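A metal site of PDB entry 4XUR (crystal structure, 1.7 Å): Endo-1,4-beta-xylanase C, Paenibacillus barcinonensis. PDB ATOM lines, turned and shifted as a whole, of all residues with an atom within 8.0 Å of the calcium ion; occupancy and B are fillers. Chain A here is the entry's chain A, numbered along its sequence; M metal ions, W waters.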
ATOM      1  N   ALA A  18      -9.925 -18.246  24.926  1.00  0.00           N
ATOM      2  CA  ALA A  18      -9.471 -17.876  26.213  1.00  0.00           C
ATOM      3  C   ALA A  18      -8.546 -16.646  26.222  1.00  0.00           C
ATOM      4  O   ALA A  18      -7.465 -16.690  25.651  1.00  0.00           O
ATOM      5  CB  ALA A  18      -8.761 -19.073  26.914  1.00  0.00           C
ATOM      6  N   ASP A  19      -9.033 -15.569  26.841  1.00  0.00           N
ATOM      7  CA  ASP A  19      -8.255 -14.331  26.880  1.00  0.00           C
ATOM      8  C   ASP A  19      -7.867 -13.979  28.323  1.00  0.00           C
ATOM      9  O   ASP A  19      -7.098 -13.067  28.532  1.00  0.00           O
ATOM     10  CB  ASP A  19      -8.961 -13.164  26.176  1.00  0.00           C
ATOM     11  CG  ASP A  19     -10.304 -12.782  26.859  1.00  0.00           C
ATOM     12  OD1 ASP A  19     -10.513 -13.066  28.050  1.00  0.00           O
ATOM     13  OD2 ASP A  19     -11.144 -12.199  26.189  1.00  0.00           O
ATOM     14  N   PHE A  20      -8.385 -14.764  29.301  1.00  0.00           N
ATOM     15  CA  PHE A  20      -8.061 -14.623  30.713  1.00  0.00           C
ATOM     16  C   PHE A  20      -8.362 -13.276  31.355  1.00  0.00           C
ATOM     17  O   PHE A  20      -7.981 -13.045  32.490  1.00  0.00           O
ATOM     18  CB  PHE A  20      -6.571 -14.981  30.969  1.00  0.00           C
ATOM     19  CG  PHE A  20      -6.240 -16.330  30.440  1.00  0.00           C
ATOM     20  CD1 PHE A  20      -6.685 -17.462  31.146  1.00  0.00           C
ATOM     21  CD2 PHE A  20      -5.570 -16.467  29.296  1.00  0.00           C
ATOM     22  CE1 PHE A  20      -6.459 -18.737  30.637  1.00  0.00           C
ATOM     23  CE2 PHE A  20      -5.286 -17.770  28.753  1.00  0.00           C
ATOM     24  CZ  PHE A  20      -5.732 -18.872  29.430  1.00  0.00           C
ATOM     25  N   GLU A  21      -9.179 -12.483  30.703  1.00  0.00           N
ATOM     26  CA  GLU A  21      -9.392 -11.092  31.159  1.00  0.00           C
ATOM     27  C   GLU A  21     -10.329 -11.036  32.338  1.00  0.00           C
ATOM     28  O   GLU A  21     -10.309 -10.024  33.108  1.00  0.00           O
ATOM     29  CB  GLU A  21      -9.871 -10.240  29.994  1.00  0.00           C
ATOM     30  CG  GLU A  21      -8.810  -9.959  28.936  1.00  0.00           C
ATOM     31  CD  GLU A  21      -7.473  -9.434  29.484  1.00  0.00           C
ATOM     32  OE1 GLU A  21      -7.471  -8.369  30.157  1.00  0.00           O
ATOM     33  OE2 GLU A  21      -6.405 -10.049  29.253  1.00  0.00           O
ATOM     34  N   ASP A  22     -11.174 -12.068  32.490  1.00  0.00           N
ATOM     35  CA  ASP A  22     -11.989 -12.257  33.675  1.00  0.00           C
ATOM     36  C   ASP A  22     -11.233 -12.750  34.924  1.00  0.00           C
ATOM     37  O   ASP A  22     -11.862 -12.918  35.972  1.00  0.00           O
ATOM     38  CB  ASP A  22     -13.164 -13.219  33.374  1.00  0.00           C
ATOM     39  CG  ASP A  22     -12.717 -14.605  32.865  1.00  0.00           C
ATOM     40  OD1 ASP A  22     -11.524 -14.993  33.058  1.00  0.00           O
ATOM     41  OD2 ASP A  22     -13.543 -15.317  32.249  1.00  0.00           O
ATOM     42  N   VAL A  38      -3.334 -17.167  36.777  1.00  0.00           N
ATOM     43  CA  VAL A  38      -3.691 -16.033  35.940  1.00  0.00           C
ATOM     44  C   VAL A  38      -3.152 -14.742  36.576  1.00  0.00           C
ATOM     45  O   VAL A  38      -3.567 -14.377  37.692  1.00  0.00           O
ATOM     46  CB  VAL A  38      -5.236 -15.910  35.786  1.00  0.00           C
ATOM     47  CG1 VAL A  38      -5.612 -14.740  34.888  1.00  0.00           C
ATOM     48  CG2 VAL A  38      -5.827 -17.200  35.227  1.00  0.00           C
ATOM     49  N   VAL A  39      -2.242 -14.083  35.880  1.00  0.00           N
ATOM     50  CA  VAL A  39      -1.542 -12.920  36.426  1.00  0.00           C
ATOM     51  C   VAL A  39      -2.128 -11.668  35.772  1.00  0.00           C
ATOM     52  O   VAL A  39      -2.746 -11.744  34.736  1.00  0.00           O
ATOM     53  CB  VAL A  39      -0.020 -12.958  36.129  1.00  0.00           C
ATOM     54  CG1 VAL A  39       0.610 -14.182  36.744  1.00  0.00           C
ATOM     55  CG2 VAL A  39       0.283 -12.812  34.637  1.00  0.00           C
ATOM     56  N   ILE A  42       0.570  -8.484  32.812  1.00  0.00           N
ATOM     57  CA  ILE A  42       1.332  -9.163  31.746  1.00  0.00           C
ATOM     58  C   ILE A  42       0.275  -9.847  30.863  1.00  0.00           C
ATOM     59  O   ILE A  42      -0.548 -10.627  31.367  1.00  0.00           O
ATOM     60  CB  ILE A  42       2.285 -10.260  32.286  1.00  0.00           C
ATOM     61  CG1 ILE A  42       3.485  -9.614  33.023  1.00  0.00           C
ATOM     62  CG2 ILE A  42       2.775 -11.136  31.117  1.00  0.00           C
ATOM     63  CD1 ILE A  42       4.475  -8.955  32.129  1.00  0.00           C
ATOM     64  N   GLY A  43       0.296  -9.505  29.567  1.00  0.00           N
ATOM     65  CA  GLY A  43      -0.707  -9.943  28.642  1.00  0.00           C
ATOM     66  C   GLY A  43      -0.362  -9.657  27.190  1.00  0.00           C
ATOM     67  O   GLY A  43       0.487  -8.831  26.923  1.00  0.00           O
ATOM     68  N   HIS A  44      -0.999 -10.373  26.245  1.00  0.00           N
ATOM     69  CA  HIS A  44      -0.855 -10.054  24.832  1.00  0.00           C
ATOM     70  C   HIS A  44      -1.848  -8.958  24.459  1.00  0.00           C
ATOM     71  O   HIS A  44      -3.056  -9.194  24.422  1.00  0.00           O
ATOM     72  CB  HIS A  44      -1.086 -11.291  23.892  1.00  0.00           C
ATOM     73  CG  HIS A  44      -1.048 -10.944  22.432  1.00  0.00           C
ATOM     74  ND1 HIS A  44       0.059 -10.368  21.795  1.00  0.00           N
ATOM     75  CD2 HIS A  44      -1.985 -11.122  21.474  1.00  0.00           C
ATOM     76  CE1 HIS A  44      -0.227 -10.227  20.505  1.00  0.00           C
ATOM     77  NE2 HIS A  44      -1.463 -10.652  20.292  1.00  0.00           N
ATOM     78  N   ASN A  45      -1.340  -7.748  24.312  1.00  0.00           N
ATOM     79  CA  ASN A  45      -2.187  -6.572  24.087  1.00  0.00           C
ATOM     80  C   ASN A  45      -3.358  -6.501  25.104  1.00  0.00           C
ATOM     81  O   ASN A  45      -4.498  -6.169  24.752  1.00  0.00           O
ATOM     82  CB  ASN A  45      -2.728  -6.567  22.659  1.00  0.00           C
ATOM     83  CG  ASN A  45      -1.664  -6.397  21.568  1.00  0.00           C
ATOM     84  OD1 ASN A  45      -1.772  -6.994  20.509  1.00  0.00           O
ATOM     85  ND2 ASN A  45      -0.673  -5.575  21.811  1.00  0.00           N
ATOM     86  N   SER A  46      -3.056  -6.805  26.358  1.00  0.00           N
ATOM     87  CA  SER A  46      -4.070  -6.887  27.418  1.00  0.00           C
ATOM     88  C   SER A  46      -3.387  -6.970  28.747  1.00  0.00           C
ATOM     89  O   SER A  46      -2.167  -6.991  28.823  1.00  0.00           O
ATOM     90  CB  SER A  46      -4.985  -8.072  27.208  1.00  0.00           C
ATOM     91  OG  SER A  46      -4.263  -9.340  27.122  1.00  0.00           O
ATOM     92  N   ASN A  47      -4.198  -7.057  29.793  1.00  0.00           N
ATOM     93  CA  ASN A  47      -3.717  -7.027  31.146  1.00  0.00           C
ATOM     94  C   ASN A  47      -3.548  -8.358  31.828  1.00  0.00           C
ATOM     95  O   ASN A  47      -2.884  -8.445  32.885  1.00  0.00           O
ATOM     96  CB  ASN A  47      -4.655  -6.108  31.987  1.00  0.00           C
ATOM     97  CG  ASN A  47      -4.057  -5.763  33.359  1.00  0.00           C
ATOM     98  OD1 ASN A  47      -2.949  -5.240  33.457  1.00  0.00           O
ATOM     99  ND2 ASN A  47      -4.817  -6.059  34.425  1.00  0.00           N
ATOM    100  N   ARG A  48      -4.115  -9.428  31.269  1.00  0.00           N
ATOM    101  CA  ARG A  48      -4.071 -10.716  31.933  1.00  0.00           C
ATOM    102  C   ARG A  48      -3.695 -11.853  30.974  1.00  0.00           C
ATOM    103  O   ARG A  48      -3.996 -11.788  29.769  1.00  0.00           O
ATOM    104  CB  ARG A  48      -5.402 -11.020  32.617  1.00  0.00           C
ATOM    105  CG  ARG A  48      -5.807  -9.905  33.608  1.00  0.00           C
ATOM    106  CD  ARG A  48      -6.800 -10.313  34.639  1.00  0.00           C
ATOM    107  NE  ARG A  48      -7.265  -9.125  35.383  1.00  0.00           N
ATOM    108  CZ  ARG A  48      -8.254  -9.133  36.269  1.00  0.00           C
ATOM    109  NH1 ARG A  48      -8.878 -10.252  36.579  1.00  0.00           N
ATOM    110  NH2 ARG A  48      -8.595  -7.992  36.861  1.00  0.00           N
ATOM    111  N   SER A  49      -3.038 -12.856  31.557  1.00  0.00           N
ATOM    112  CA  SER A  49      -2.577 -14.023  30.756  1.00  0.00           C
ATOM    113  C   SER A  49      -2.297 -15.154  31.702  1.00  0.00           C
ATOM    114  O   SER A  49      -2.412 -15.019  32.886  1.00  0.00           O
ATOM    115  CB  SER A  49      -1.363 -13.614  29.928  1.00  0.00           C
ATOM    116  OG  SER A  49      -0.256 -13.292  30.754  1.00  0.00           O
ATOM    117  N   LEU A  50      -1.914 -16.329  31.162  1.00  0.00           N
ATOM    118  CA  LEU A  50      -1.739 -17.490  31.987  1.00  0.00           C
ATOM    119  C   LEU A  50      -0.277 -17.802  32.075  1.00  0.00           C
ATOM    120  O   LEU A  50       0.357 -18.152  31.090  1.00  0.00           O
ATOM    121  CB  LEU A  50      -2.475 -18.685  31.345  1.00  0.00           C
ATOM    122  CG  LEU A  50      -2.379 -19.993  32.147  1.00  0.00           C
ATOM    123  CD1 LEU A  50      -2.850 -19.808  33.573  1.00  0.00           C
ATOM    124  CD2 LEU A  50      -3.152 -21.063  31.386  1.00  0.00           C
ATOM    125  N   TRP A 123       5.932 -11.416  22.383  1.00  0.00           N
ATOM    126  CA  TRP A 123       4.742 -12.251  22.078  1.00  0.00           C
ATOM    127  C   TRP A 123       4.718 -12.733  20.655  1.00  0.00           C
ATOM    128  O   TRP A 123       4.950 -11.949  19.673  1.00  0.00           O
ATOM    129  CB  TRP A 123       3.472 -11.497  22.358  1.00  0.00           C
ATOM    130  CG  TRP A 123       3.223 -11.236  23.823  1.00  0.00           C
ATOM    131  CD1 TRP A 123       3.516 -10.141  24.492  1.00  0.00           C
ATOM    132  CD2 TRP A 123       2.581 -12.125  24.742  1.00  0.00           C
ATOM    133  NE1 TRP A 123       3.150 -10.251  25.808  1.00  0.00           N
ATOM    134  CE2 TRP A 123       2.554 -11.481  25.996  1.00  0.00           C
ATOM    135  CE3 TRP A 123       2.068 -13.417  24.634  1.00  0.00           C
ATOM    136  CZ2 TRP A 123       2.022 -12.055  27.125  1.00  0.00           C
ATOM    137  CZ3 TRP A 123       1.567 -14.026  25.780  1.00  0.00           C
ATOM    138  CH2 TRP A 123       1.509 -13.371  26.983  1.00  0.00           C
ATOM    139  N   VAL A 166       0.981 -17.814  28.277  1.00  0.00           N
ATOM    140  CA  VAL A 166       0.149 -17.937  27.083  1.00  0.00           C
ATOM    141  C   VAL A 166      -1.101 -17.056  27.182  1.00  0.00           C
ATOM    142  O   VAL A 166      -1.517 -16.729  28.290  1.00  0.00           O
ATOM    143  CB  VAL A 166      -0.350 -19.383  26.775  1.00  0.00           C
ATOM    144  CG1 VAL A 166       0.840 -20.331  26.583  1.00  0.00           C
ATOM    145  CG2 VAL A 166      -1.254 -19.920  27.858  1.00  0.00           C
ATOM    146  N   ASP A 167      -1.631 -16.645  26.049  1.00  0.00           N
ATOM    147  CA  ASP A 167      -2.796 -15.762  25.963  1.00  0.00           C
ATOM    148  C   ASP A 167      -3.512 -15.926  24.620  1.00  0.00           C
ATOM    149  O   ASP A 167      -2.970 -16.486  23.670  1.00  0.00           O
ATOM    150  CB  ASP A 167      -2.358 -14.287  26.159  1.00  0.00           C
ATOM    151  CG  ASP A 167      -3.442 -13.389  26.668  1.00  0.00           C
ATOM    152  OD1 ASP A 167      -4.561 -13.827  27.071  1.00  0.00           O
ATOM    153  OD2 ASP A 167      -3.143 -12.165  26.707  1.00  0.00           O
ATOM    154  N   ASP A 168      -4.759 -15.453  24.557  1.00  0.00           N
ATOM    155  CA  ASP A 168      -5.521 -15.373  23.301  1.00  0.00           C
ATOM    156  C   ASP A 168      -5.580 -16.727  22.547  1.00  0.00           C
ATOM    157  O   ASP A 168      -5.269 -16.800  21.337  1.00  0.00           O
ATOM    158  CB  ASP A 168      -5.010 -14.242  22.396  1.00  0.00           C
ATOM    159  CG  ASP A 168      -5.370 -12.852  22.945  1.00  0.00           C
ATOM    160  OD1 ASP A 168      -6.340 -12.710  23.762  1.00  0.00           O
ATOM    161  OD2 ASP A 168      -4.650 -11.878  22.578  1.00  0.00           O
ATOM    162  N   VAL A 169      -5.946 -17.766  23.270  1.00  0.00           N
ATOM    163  CA  VAL A 169      -6.093 -19.124  22.733  1.00  0.00           C
ATOM    164  C   VAL A 169      -7.442 -19.153  22.019  1.00  0.00           C
ATOM    165  O   VAL A 169      -8.462 -18.721  22.587  1.00  0.00           O
ATOM    166  CB  VAL A 169      -6.113 -20.178  23.837  1.00  0.00           C
ATOM    167  CG1 VAL A 169      -6.242 -21.543  23.208  1.00  0.00           C
ATOM    168  CG2 VAL A 169      -4.846 -20.125  24.682  1.00  0.00           C
HETATM  169 CA    CA M   1      -5.314 -11.624  27.887  1.00  0.00          CA
HETATM  170  O   HOH W   1      -6.245 -11.019  25.979  1.00  0.00           O
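OD2 of Asp 167 lies close to N of His 44, at 2.8 Å.
The side-chain hydroxyl (OG) of Ser 46 lies close to the backbone carbonyl oxygen (O) of His 44 (3.0 Å).
Of the 21 residues printed, 5 come within 4 Å of the calcium ion.
The calcium ion is bound by water W1 (2.2 Å), the backbone carbonyl oxygen (O) of Arg 48 (2.3 Å), the side-chain carboxylate (OE2) of Glu 21 (2.4 Å), the backbone carbonyl oxygen (O) of Asp 19 (2.4 Å), the side-chain carboxylate (OD1) of Asp 167 (2.5 Å), the side-chain carboxylate (OD2) of Asp 167 (2.5 Å) and the side-chain hydroxyl (OG) of Ser 46 (2.6 Å).
The calcium ion has seven donor atoms within binding distance.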
